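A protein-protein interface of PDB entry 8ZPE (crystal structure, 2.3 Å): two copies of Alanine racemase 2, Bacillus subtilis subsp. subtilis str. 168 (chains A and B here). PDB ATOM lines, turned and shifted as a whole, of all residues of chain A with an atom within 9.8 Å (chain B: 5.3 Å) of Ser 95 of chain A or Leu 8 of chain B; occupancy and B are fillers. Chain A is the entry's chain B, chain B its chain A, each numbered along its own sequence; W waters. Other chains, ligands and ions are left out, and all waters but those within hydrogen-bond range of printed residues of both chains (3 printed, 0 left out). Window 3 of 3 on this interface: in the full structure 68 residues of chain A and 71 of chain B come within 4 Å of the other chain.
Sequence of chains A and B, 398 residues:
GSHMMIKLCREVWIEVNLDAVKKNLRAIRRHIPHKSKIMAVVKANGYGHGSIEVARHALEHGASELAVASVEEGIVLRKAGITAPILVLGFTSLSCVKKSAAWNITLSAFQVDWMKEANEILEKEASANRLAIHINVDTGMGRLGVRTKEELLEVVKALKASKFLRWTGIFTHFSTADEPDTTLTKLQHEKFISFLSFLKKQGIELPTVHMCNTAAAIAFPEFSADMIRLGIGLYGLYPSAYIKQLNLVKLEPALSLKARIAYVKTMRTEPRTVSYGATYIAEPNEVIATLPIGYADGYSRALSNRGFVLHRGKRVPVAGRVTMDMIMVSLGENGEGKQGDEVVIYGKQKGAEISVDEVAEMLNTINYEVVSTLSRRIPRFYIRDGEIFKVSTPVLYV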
ATOM      1  N   SER A  70       5.543  13.556   6.518  1.00  0.00           N
ATOM      2  CA  SER A  70       4.929  12.659   7.481  1.00  0.00           C
ATOM      3  C   SER A  70       5.371  13.075   8.873  1.00  0.00           C
ATOM      4  O   SER A  70       6.359  13.800   9.045  1.00  0.00           O
ATOM      5  CB  SER A  70       5.357  11.222   7.229  1.00  0.00           C
ATOM      6  OG  SER A  70       6.737  11.117   7.525  1.00  0.00           O
ATOM      7  N   VAL A  71       4.650  12.554   9.872  1.00  0.00           N
ATOM      8  CA  VAL A  71       5.011  12.802  11.262  1.00  0.00           C
ATOM      9  C   VAL A  71       6.371  12.199  11.564  1.00  0.00           C
ATOM     10  O   VAL A  71       7.175  12.783  12.303  1.00  0.00           O
ATOM     11  CB  VAL A  71       3.924  12.236  12.190  1.00  0.00           C
ATOM     12  CG1 VAL A  71       4.441  12.143  13.646  1.00  0.00           C
ATOM     13  CG2 VAL A  71       2.675  13.086  12.099  1.00  0.00           C
ATOM     14  N   GLU A  72       6.638  11.002  11.019  1.00  0.00           N
ATOM     15  CA  GLU A  72       7.940  10.358  11.192  1.00  0.00           C
ATOM     16  C   GLU A  72       9.084  11.269  10.733  1.00  0.00           C
ATOM     17  O   GLU A  72      10.121  11.366  11.399  1.00  0.00           O
ATOM     18  CB  GLU A  72       7.976   9.014  10.431  1.00  0.00           C
ATOM     19  CG  GLU A  72       6.975   7.936  10.911  1.00  0.00           C
ATOM     20  CD  GLU A  72       5.586   8.072  10.267  1.00  0.00           C
ATOM     21  OE1 GLU A  72       5.221   9.197   9.877  1.00  0.00           O
ATOM     22  OE2 GLU A  72       4.842   7.061  10.164  1.00  0.00           O
ATOM     23  N   PHE A  91      -1.306  13.360   4.556  1.00  0.00           N
ATOM     24  CA  PHE A  91      -2.381  12.969   5.445  1.00  0.00           C
ATOM     25  C   PHE A  91      -1.799  12.184   6.615  1.00  0.00           C
ATOM     26  O   PHE A  91      -1.002  11.256   6.424  1.00  0.00           O
ATOM     27  CB  PHE A  91      -3.417  12.135   4.688  1.00  0.00           C
ATOM     28  CG  PHE A  91      -4.500  11.577   5.568  1.00  0.00           C
ATOM     29  CD1 PHE A  91      -5.572  12.371   5.958  1.00  0.00           C
ATOM     30  CD2 PHE A  91      -4.436  10.253   6.019  1.00  0.00           C
ATOM     31  CE1 PHE A  91      -6.570  11.856   6.773  1.00  0.00           C
ATOM     32  CE2 PHE A  91      -5.421   9.721   6.832  1.00  0.00           C
ATOM     33  CZ  PHE A  91      -6.499  10.521   7.212  1.00  0.00           C
ATOM     34  N   THR A  92      -2.195  12.549   7.826  1.00  0.00           N
ATOM     35  CA  THR A  92      -1.758  11.843   9.015  1.00  0.00           C
ATOM     36  C   THR A  92      -2.938  11.095   9.608  1.00  0.00           C
ATOM     37  O   THR A  92      -3.995  11.684   9.867  1.00  0.00           O
ATOM     38  CB  THR A  92      -1.149  12.798  10.031  1.00  0.00           C
ATOM     39  OG1 THR A  92       0.017  13.403   9.460  1.00  0.00           O
ATOM     40  CG2 THR A  92      -0.771  12.060  11.315  1.00  0.00           C
ATOM     41  N   SER A  93      -2.749   9.794   9.795  1.00  0.00           N
ATOM     42  CA  SER A  93      -3.743   8.961  10.447  1.00  0.00           C
ATOM     43  C   SER A  93      -4.134   9.522  11.810  1.00  0.00           C
ATOM     44  O   SER A  93      -3.310  10.092  12.522  1.00  0.00           O
ATOM     45  CB  SER A  93      -3.180   7.545  10.593  1.00  0.00           C
ATOM     46  OG  SER A  93      -3.647   6.930  11.781  1.00  0.00           O
ATOM     47  N   LEU A  94      -5.402   9.330  12.172  1.00  0.00           N
ATOM     48  CA  LEU A  94      -5.862   9.649  13.514  1.00  0.00           C
ATOM     49  C   LEU A  94      -5.074   8.894  14.571  1.00  0.00           C
ATOM     50  O   LEU A  94      -4.966   9.355  15.709  1.00  0.00           O
ATOM     51  CB  LEU A  94      -7.361   9.341  13.642  1.00  0.00           C
ATOM     52  CG  LEU A  94      -8.275  10.387  12.984  1.00  0.00           C
ATOM     53  CD1 LEU A  94      -9.699   9.912  12.970  1.00  0.00           C
ATOM     54  CD2 LEU A  94      -8.180  11.744  13.678  1.00  0.00           C
ATOM     55  N   SER A  95      -4.500   7.748  14.223  1.00  0.00           N
ATOM     56  CA  SER A  95      -3.751   7.051  15.256  1.00  0.00           C
ATOM     57  C   SER A  95      -2.469   7.777  15.637  1.00  0.00           C
ATOM     58  O   SER A  95      -1.790   7.345  16.574  1.00  0.00           O
ATOM     59  CB  SER A  95      -3.449   5.617  14.806  1.00  0.00           C
ATOM     60  OG  SER A  95      -2.535   5.620  13.731  1.00  0.00           O
ATOM     61  N   CYS A  96      -2.117   8.870  14.964  1.00  0.00           N
ATOM     62  CA  CYS A  96      -0.932   9.634  15.342  1.00  0.00           C
ATOM     63  C   CYS A  96      -1.252  11.025  15.872  1.00  0.00           C
ATOM     64  O   CYS A  96      -0.335  11.848  15.984  1.00  0.00           O
ATOM     65  CB  CYS A  96       0.037   9.746  14.166  1.00  0.00           C
ATOM     66  SG  CYS A  96       0.902   8.214  13.861  1.00  0.00           S
ATOM     67  N   VAL A  97      -2.509  11.310  16.225  1.00  0.00           N
ATOM     68  CA  VAL A  97      -2.845  12.646  16.733  1.00  0.00           C
ATOM     69  C   VAL A  97      -2.116  12.931  18.040  1.00  0.00           C
ATOM     70  O   VAL A  97      -1.528  14.006  18.216  1.00  0.00           O
ATOM     71  CB  VAL A  97      -4.366  12.812  16.885  1.00  0.00           C
ATOM     72  CG1 VAL A  97      -4.695  13.821  17.965  1.00  0.00           C
ATOM     73  CG2 VAL A  97      -4.954  13.283  15.578  1.00  0.00           C
ATOM     74  N   LYS A  98      -2.125  11.973  18.972  1.00  0.00           N
ATOM     75  CA  LYS A  98      -1.507  12.200  20.276  1.00  0.00           C
ATOM     76  C   LYS A  98       0.008  12.380  20.156  1.00  0.00           C
ATOM     77  O   LYS A  98       0.604  13.246  20.822  1.00  0.00           O
ATOM     78  CB  LYS A  98      -1.846  11.038  21.218  1.00  0.00           C
ATOM     79  CG  LYS A  98      -1.000  11.005  22.491  1.00  0.00           C
ATOM     80  CD  LYS A  98      -1.724  10.338  23.660  1.00  0.00           C
ATOM     81  CE  LYS A  98      -0.813  10.201  24.901  1.00  0.00           C
ATOM     82  NZ  LYS A  98      -0.803  11.404  25.822  1.00  0.00           N
ATOM     83  N   LYS A  99       0.651  11.552  19.326  1.00  0.00           N
ATOM     84  CA  LYS A  99       2.083  11.678  19.106  1.00  0.00           C
ATOM     85  C   LYS A  99       2.416  13.017  18.473  1.00  0.00           C
ATOM     86  O   LYS A  99       3.426  13.641  18.814  1.00  0.00           O
ATOM     87  CB  LYS A  99       2.573  10.538  18.219  1.00  0.00           C
ATOM     88  CG  LYS A  99       4.028  10.238  18.383  1.00  0.00           C
ATOM     89  CD  LYS A  99       4.602   9.528  17.170  1.00  0.00           C
ATOM     90  CE  LYS A  99       3.792   8.297  16.790  1.00  0.00           C
ATOM     91  NZ  LYS A  99       4.547   7.426  15.823  1.00  0.00           N
ATOM     92  N   SER A 100       1.580  13.474  17.537  1.00  0.00           N
ATOM     93  CA  SER A 100       1.830  14.769  16.910  1.00  0.00           C
ATOM     94  C   SER A 100       1.705  15.900  17.912  1.00  0.00           C
ATOM     95  O   SER A 100       2.430  16.891  17.818  1.00  0.00           O
ATOM     96  CB  SER A 100       0.866  14.996  15.749  1.00  0.00           C
ATOM     97  OG  SER A 100       1.024  13.986  14.765  1.00  0.00           O
ATOM     98  N   ALA A 101       0.794  15.771  18.873  1.00  0.00           N
ATOM     99  CA  ALA A 101       0.676  16.792  19.903  1.00  0.00           C
ATOM    100  C   ALA A 101       1.858  16.750  20.864  1.00  0.00           C
ATOM    101  O   ALA A 101       2.313  17.795  21.322  1.00  0.00           O
ATOM    102  CB  ALA A 101      -0.650  16.630  20.646  1.00  0.00           C
ATOM    103  N   LEU A 107      -0.079  19.487  11.760  1.00  0.00           N
ATOM    104  CA  LEU A 107      -0.648  18.587  10.766  1.00  0.00           C
ATOM    105  C   LEU A 107      -1.559  19.370   9.834  1.00  0.00           C
ATOM    106  O   LEU A 107      -2.177  20.360  10.231  1.00  0.00           O
ATOM    107  CB  LEU A 107      -1.440  17.455  11.432  1.00  0.00           C
ATOM    108  CG  LEU A 107      -0.724  16.670  12.539  1.00  0.00           C
ATOM    109  CD1 LEU A 107      -1.664  15.677  13.186  1.00  0.00           C
ATOM    110  CD2 LEU A 107       0.470  15.933  11.956  1.00  0.00           C
ATOM    111  N   TRP A 114     -12.384  14.324  10.731  1.00  0.00           N
ATOM    112  CA  TRP A 114     -11.018  14.225  11.220  1.00  0.00           C
ATOM    113  C   TRP A 114     -10.760  15.236  12.347  1.00  0.00           C
ATOM    114  O   TRP A 114     -10.260  14.867  13.420  1.00  0.00           O
ATOM    115  CB  TRP A 114     -10.064  14.404  10.033  1.00  0.00           C
ATOM    116  CG  TRP A 114      -8.677  13.957  10.298  1.00  0.00           C
ATOM    117  CD1 TRP A 114      -8.122  12.754   9.975  1.00  0.00           C
ATOM    118  CD2 TRP A 114      -7.654  14.712  10.960  1.00  0.00           C
ATOM    119  NE1 TRP A 114      -6.808  12.714  10.391  1.00  0.00           N
ATOM    120  CE2 TRP A 114      -6.501  13.901  11.007  1.00  0.00           C
ATOM    121  CE3 TRP A 114      -7.603  15.997  11.520  1.00  0.00           C
ATOM    122  CZ2 TRP A 114      -5.312  14.329  11.578  1.00  0.00           C
ATOM    123  CZ3 TRP A 114      -6.422  16.418  12.099  1.00  0.00           C
ATOM    124  CH2 TRP A 114      -5.286  15.586  12.119  1.00  0.00           C
ATOM    125  N   GLU A 117     -12.769  14.096  15.439  1.00  0.00           N
ATOM    126  CA  GLU A 117     -12.099  12.931  16.009  1.00  0.00           C
ATOM    127  C   GLU A 117     -10.745  13.299  16.599  1.00  0.00           C
ATOM    128  O   GLU A 117     -10.391  12.822  17.682  1.00  0.00           O
ATOM    129  CB  GLU A 117     -11.939  11.844  14.947  1.00  0.00           C
ATOM    130  CG  GLU A 117     -13.230  11.140  14.596  1.00  0.00           C
ATOM    131  CD  GLU A 117     -13.695  10.229  15.708  1.00  0.00           C
ATOM    132  OE1 GLU A 117     -12.823   9.576  16.333  1.00  0.00           O
ATOM    133  OE2 GLU A 117     -14.920  10.169  15.966  1.00  0.00           O
ATOM    134  N   ALA A 118      -9.961  14.133  15.902  1.00  0.00           N
ATOM    135  CA  ALA A 118      -8.667  14.529  16.455  1.00  0.00           C
ATOM    136  C   ALA A 118      -8.845  15.281  17.762  1.00  0.00           C
ATOM    137  O   ALA A 118      -8.095  15.065  18.723  1.00  0.00           O
ATOM    138  CB  ALA A 118      -7.884  15.389  15.458  1.00  0.00           C
ATOM    139  N   ILE A 121      -9.824  12.963  20.685  1.00  0.00           N
ATOM    140  CA  ILE A 121      -8.672  12.166  21.101  1.00  0.00           C
ATOM    141  C   ILE A 121      -7.826  12.929  22.112  1.00  0.00           C
ATOM    142  O   ILE A 121      -7.430  12.385  23.147  1.00  0.00           O
ATOM    143  CB  ILE A 121      -7.833  11.751  19.884  1.00  0.00           C
ATOM    144  CG1 ILE A 121      -8.527  10.623  19.113  1.00  0.00           C
ATOM    145  CG2 ILE A 121      -6.423  11.384  20.349  1.00  0.00           C
ATOM    146  CD1 ILE A 121      -7.913  10.343  17.747  1.00  0.00           C
ATOM    147  N   LEU A 122      -7.511  14.196  21.813  1.00  0.00           N
ATOM    148  CA  LEU A 122      -6.739  15.007  22.752  1.00  0.00           C
ATOM    149  C   LEU A 122      -7.583  15.417  23.951  1.00  0.00           C
ATOM    150  O   LEU A 122      -7.054  15.605  25.051  1.00  0.00           O
ATOM    151  CB  LEU A 122      -6.172  16.247  22.054  1.00  0.00           C
ATOM    152  CG  LEU A 122      -5.271  15.929  20.866  1.00  0.00           C
ATOM    153  CD1 LEU A 122      -4.799  17.176  20.137  1.00  0.00           C
ATOM    154  CD2 LEU A 122      -4.104  15.058  21.295  1.00  0.00           C
ATOM    155  N   GLU A 125      -7.664  12.713  26.533  1.00  0.00           N
ATOM    156  CA  GLU A 125      -6.365  12.552  27.168  1.00  0.00           C
ATOM    157  C   GLU A 125      -5.987  13.757  28.022  1.00  0.00           C
ATOM    158  O   GLU A 125      -4.851  13.822  28.510  1.00  0.00           O
ATOM    159  CB  GLU A 125      -5.287  12.285  26.115  1.00  0.00           C
ATOM    160  CG  GLU A 125      -5.262  10.839  25.592  1.00  0.00           C
ATOM    161  CD  GLU A 125      -4.147  10.008  26.212  1.00  0.00           C
ATOM    162  OE1 GLU A 125      -3.566  10.431  27.238  1.00  0.00           O
ATOM    163  OE2 GLU A 125      -3.847   8.932  25.669  1.00  0.00           O
ATOM    164  N   LEU A 131      -3.018  20.884  19.403  1.00  0.00           N
ATOM    165  CA  LEU A 131      -2.468  20.426  18.132  1.00  0.00           C
ATOM    166  C   LEU A 131      -2.615  21.494  17.042  1.00  0.00           C
ATOM    167  O   LEU A 131      -3.733  21.827  16.628  1.00  0.00           O
ATOM    168  CB  LEU A 131      -3.175  19.142  17.715  1.00  0.00           C
ATOM    169  CG  LEU A 131      -2.692  18.547  16.394  1.00  0.00           C
ATOM    170  CD1 LEU A 131      -1.247  18.082  16.560  1.00  0.00           C
ATOM    171  CD2 LEU A 131      -3.604  17.401  15.907  1.00  0.00           C
ATOM    172  N   ILE B   6      -1.769  -2.629  11.706  1.00  0.00           N
ATOM    173  CA  ILE B   6      -0.593  -1.795  11.486  1.00  0.00           C
ATOM    174  C   ILE B   6      -0.980  -0.336  11.695  1.00  0.00           C
ATOM    175  O   ILE B   6      -1.871   0.176  11.018  1.00  0.00           O
ATOM    176  CB  ILE B   6      -0.024  -2.036  10.079  1.00  0.00           C
ATOM    177  CG1 ILE B   6       0.344  -3.514   9.918  1.00  0.00           C
ATOM    178  CG2 ILE B   6       1.150  -1.117   9.786  1.00  0.00           C
ATOM    179  CD1 ILE B   6      -0.134  -4.124   8.643  1.00  0.00           C
ATOM    180  N   LYS B   7      -0.333   0.325  12.650  1.00  0.00           N
ATOM    181  CA  LYS B   7      -0.638   1.711  12.997  1.00  0.00           C
ATOM    182  C   LYS B   7       0.532   2.581  12.558  1.00  0.00           C
ATOM    183  O   LYS B   7       1.611   2.542  13.157  1.00  0.00           O
ATOM    184  CB  LYS B   7      -0.923   1.872  14.491  1.00  0.00           C
ATOM    185  CG  LYS B   7      -2.335   1.422  14.889  1.00  0.00           C
ATOM    186  CD  LYS B   7      -2.381   0.873  16.315  1.00  0.00           C
ATOM    187  CE  LYS B   7      -1.332  -0.222  16.541  1.00  0.00           C
ATOM    188  NZ  LYS B   7      -0.944  -0.366  17.981  1.00  0.00           N
ATOM    189  N   LEU B   8       0.319   3.346  11.503  1.00  0.00           N
ATOM    190  CA  LEU B   8       1.300   4.285  11.006  1.00  0.00           C
ATOM    191  C   LEU B   8       0.677   5.667  10.932  1.00  0.00           C
ATOM    192  O   LEU B   8      -0.544   5.812  10.803  1.00  0.00           O
ATOM    193  CB  LEU B   8       1.802   3.860   9.628  1.00  0.00           C
ATOM    194  CG  LEU B   8       2.259   2.413   9.601  1.00  0.00           C
ATOM    195  CD1 LEU B   8       2.482   1.973   8.176  1.00  0.00           C
ATOM    196  CD2 LEU B   8       3.520   2.311  10.435  1.00  0.00           C
ATOM    197  N   CYS B   9       1.526   6.685  11.034  1.00  0.00           N
ATOM    198  CA  CYS B   9       1.080   8.029  10.709  1.00  0.00           C
ATOM    199  C   CYS B   9       0.892   8.155   9.204  1.00  0.00           C
ATOM    200  O   CYS B   9      -0.177   8.552   8.722  1.00  0.00           O
ATOM    201  CB  CYS B   9       2.094   9.053  11.229  1.00  0.00           C
ATOM    202  SG  CYS B   9       2.631   8.769  12.949  1.00  0.00           S
ATOM    203  N   ARG B  10       1.930   7.823   8.449  1.00  0.00           N
ATOM    204  CA  ARG B  10       1.864   7.738   7.002  1.00  0.00           C
ATOM    205  C   ARG B  10       1.646   6.269   6.669  1.00  0.00           C
ATOM    206  O   ARG B  10       2.516   5.434   6.915  1.00  0.00           O
ATOM    207  CB  ARG B  10       3.136   8.285   6.366  1.00  0.00           C
ATOM    208  CG  ARG B  10       3.084   8.424   4.870  1.00  0.00           C
ATOM    209  CD  ARG B  10       4.490   8.542   4.338  1.00  0.00           C
ATOM    210  NE  ARG B  10       4.499   8.802   2.910  1.00  0.00           N
ATOM    211  CZ  ARG B  10       5.349   8.252   2.054  1.00  0.00           C
ATOM    212  NH1 ARG B  10       6.273   7.390   2.450  1.00  0.00           N
ATOM    213  NH2 ARG B  10       5.263   8.567   0.769  1.00  0.00           N
ATOM    214  N   GLU B  11       0.480   5.954   6.124  1.00  0.00           N
ATOM    215  CA  GLU B  11       0.020   4.577   6.041  1.00  0.00           C
ATOM    216  C   GLU B  11       0.467   3.923   4.735  1.00  0.00           C
ATOM    217  O   GLU B  11      -0.338   3.590   3.861  1.00  0.00           O
ATOM    218  CB  GLU B  11      -1.487   4.545   6.185  1.00  0.00           C
ATOM    219  CG  GLU B  11      -1.966   5.404   7.318  1.00  0.00           C
ATOM    220  CD  GLU B  11      -3.413   5.178   7.598  1.00  0.00           C
ATOM    221  OE1 GLU B  11      -4.233   5.682   6.810  1.00  0.00           O
ATOM    222  OE2 GLU B  11      -3.729   4.483   8.586  1.00  0.00           O
ATOM    223  N   VAL B  12       1.782   3.728   4.627  1.00  0.00           N
ATOM    224  CA  VAL B  12       2.384   2.868   3.608  1.00  0.00           C
ATOM    225  C   VAL B  12       3.411   1.969   4.293  1.00  0.00           C
ATOM    226  O   VAL B  12       4.127   2.409   5.203  1.00  0.00           O
ATOM    227  CB  VAL B  12       3.035   3.686   2.459  1.00  0.00           C
ATOM    228  CG1 VAL B  12       4.053   4.718   2.998  1.00  0.00           C
ATOM    229  CG2 VAL B  12       3.697   2.759   1.439  1.00  0.00           C
ATOM    230  N   TRP B  13       3.496   0.718   3.852  1.00  0.00           N
ATOM    231  CA  TRP B  13       4.421  -0.206   4.490  1.00  0.00           C
ATOM    232  C   TRP B  13       4.727  -1.389   3.576  1.00  0.00           C
ATOM    233  O   TRP B  13       4.030  -1.653   2.592  1.00  0.00           O
ATOM    234  CB  TRP B  13       3.849  -0.699   5.823  1.00  0.00           C
ATOM    235  CG  TRP B  13       2.661  -1.632   5.652  1.00  0.00           C
ATOM    236  CD1 TRP B  13       2.677  -3.001   5.625  1.00  0.00           C
ATOM    237  CD2 TRP B  13       1.297  -1.247   5.486  1.00  0.00           C
ATOM    238  NE1 TRP B  13       1.400  -3.487   5.467  1.00  0.00           N
ATOM    239  CE2 TRP B  13       0.535  -2.431   5.377  1.00  0.00           C
ATOM    240  CE3 TRP B  13       0.643  -0.017   5.417  1.00  0.00           C
ATOM    241  CZ2 TRP B  13      -0.840  -2.414   5.198  1.00  0.00           C
ATOM    242  CZ3 TRP B  13      -0.712  -0.004   5.245  1.00  0.00           C
ATOM    243  CH2 TRP B  13      -1.449  -1.195   5.141  1.00  0.00           C
ATOM    244  N   PRO B 379       8.492   1.606   6.395  1.00  0.00           N
ATOM    245  CA  PRO B 379       8.719   0.573   7.405  1.00  0.00           C
ATOM    246  C   PRO B 379       8.457  -0.832   6.849  1.00  0.00           C
ATOM    247  O   PRO B 379       7.532  -1.052   6.062  1.00  0.00           O
ATOM    248  CB  PRO B 379       7.722   0.944   8.513  1.00  0.00           C
ATOM    249  CG  PRO B 379       6.608   1.665   7.777  1.00  0.00           C
ATOM    250  CD  PRO B 379       7.296   2.420   6.681  1.00  0.00           C
ATOM    251  N   PHE B 381       7.592  -4.749   7.719  1.00  0.00           N
ATOM    252  CA  PHE B 381       6.983  -5.678   8.662  1.00  0.00           C
ATOM    253  C   PHE B 381       7.251  -7.111   8.229  1.00  0.00           C
ATOM    254  O   PHE B 381       7.161  -7.435   7.047  1.00  0.00           O
ATOM    255  CB  PHE B 381       5.485  -5.433   8.758  1.00  0.00           C
ATOM    256  CG  PHE B 381       5.146  -4.152   9.432  1.00  0.00           C
ATOM    257  CD1 PHE B 381       4.999  -4.105  10.819  1.00  0.00           C
ATOM    258  CD2 PHE B 381       5.008  -2.987   8.695  1.00  0.00           C
ATOM    259  CE1 PHE B 381       4.694  -2.913  11.461  1.00  0.00           C
ATOM    260  CE2 PHE B 381       4.699  -1.791   9.328  1.00  0.00           C
ATOM    261  CZ  PHE B 381       4.534  -1.756  10.716  1.00  0.00           C
HETATM  262  O   HOH W   1      -0.941   8.187   5.257  1.00  0.00           O
HETATM  263  O   HOH W   2       4.565   5.788  12.328  1.00  0.00           O
HETATM  264  O   HOH W   3      -2.653   3.949  11.281  1.00  0.00           O
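The backbone carbonyl oxygen (O) of Leu 8 of chain B sits close to the side-chain hydroxyl (OG) of Ser 93 of chain A (3.4 Å). The side-chain carboxylate (OE2) of Glu 72 of chain A sits at hydrogen-bond distance from the backbone NH (N) of Cys 9 of chain B (3.4 Å). O of Cys 9 of chain B sits at hydrogen-bond distance from N of Ser 93 of chain A, at 3.1 Å. SG of Cys 96 of chain A is disulfide-bonded to SG of Cys 9 of chain B, 2.0 Å away. The side-chain sulfur (SG) of Cys 9 of chain B lies within hydrogen-bond range of the side-chain amino group (NZ) of Lys 99 of chain A, at 3.7 Å. The backbone NH of Arg 10 of chain B lies within hydrogen-bond range of the side-chain carboxylate of Glu 72 of chain A, 3.5 Å away.
OG of Ser 70 of chain A lies close to OE1 of Glu 72 of chain A, 3.4 Å away. The backbone carbonyl oxygen (O) of Thr 92 of chain A is in hydrogen-bond range of the indole nitrogen (NE1) of Trp 114 of chain A, 3.0 Å away. OG of Ser 93 of chain A sits at hydrogen-bond distance from OG of Ser 95 of chain A (2.6 Å). The side-chain hydroxyl of Ser 100 of chain A sits at hydrogen-bond distance from the backbone carbonyl oxygen of Cys 96 of chain A (2.8 Å).
Ser 70 of chain A touches Arg 10 of chain B. Cys 9 of chain B touches Val 71 of chain A. O of Phe 91 of chain A touches O of Cys 9 of chain B, at 3.6 Å. O of Cys 9 of chain B touches CA of Thr 92 of chain A (3.7 Å). OE2 of Glu 11 of chain B touches CB of Ser 93 of chain A, at 3.7 Å. Ser 95 of chain A touches Leu 8 of chain B. C of Leu 8 of chain B touches SG of Cys 96 of chain A, at 3.9 Å.
Of chain B, only Leu 8 (3.5 Å) comes within 4 Å of Ser 95 of chain A. Printed residues of chain A within 4 Å of Leu 8 of chain B: Ser 93 (3.2 Å), Ser 95 (3.5 Å) and Cys 96 (3.9 Å). Cys 9 of chain B touches just these residues of chain A: Val 71, Glu 72, Phe 91, Thr 92, Ser 93, Cys 96 and Lys 99. Of the printed residues of chain B, Thr 92 of chain A touches Cys 9. Printed residues of chain B within 4 Å of Cys 96 of chain A: Leu 8 and Cys 9. Of the printed residues of chain B, Phe 91 of chain A touches Cys 9 (3.6 Å). Ile 121 of chain A touches none of the printed residues of chain B. The nearest residue of chain A that does not touch Leu 8 of chain B is Glu 72 of chain A (4.4 Å).
Hydrophobic or aromatic side chains of chain A that line the printed part of chain B: Val 71. Of the 10 printed residues of chain B, 4 touch a printed residue of chain A. Printed residues of chain B that touch a printed residue of chain A: Leu 8, Cys 9, Arg 10 and Glu 11. Among the printed residues, 13 pairs touch across the chains. Among the printed residues, no Asp or Glu carboxylate lies within 4 Å of a Lys or Arg side-chain nitrogen of the other chain.
No position is printed for both chains. Of the 13 pairs that touch across the chains among the printed residues, none has its exchanged pair printed and touching as well.
Water W2 lies within hydrogen-bond range of OE2 of Glu 72 of chain A and N of Cys 9 of chain B. Water W1 bridges the backbone NH (N) of Glu 11 of chain B and the backbone carbonyl oxygen (O) of Phe 91 of chain A. Water W3 lies within hydrogen-bond range of the backbone carbonyl oxygen of Leu 8 of chain B (2.9 Å), the side-chain carboxylate of Glu 11 of chain B (3.0 Å), the side-chain hydroxyl of Ser 95 of chain A (3.0 Å) and the side-chain hydroxyl of Ser 93 of chain A (3.2 Å).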
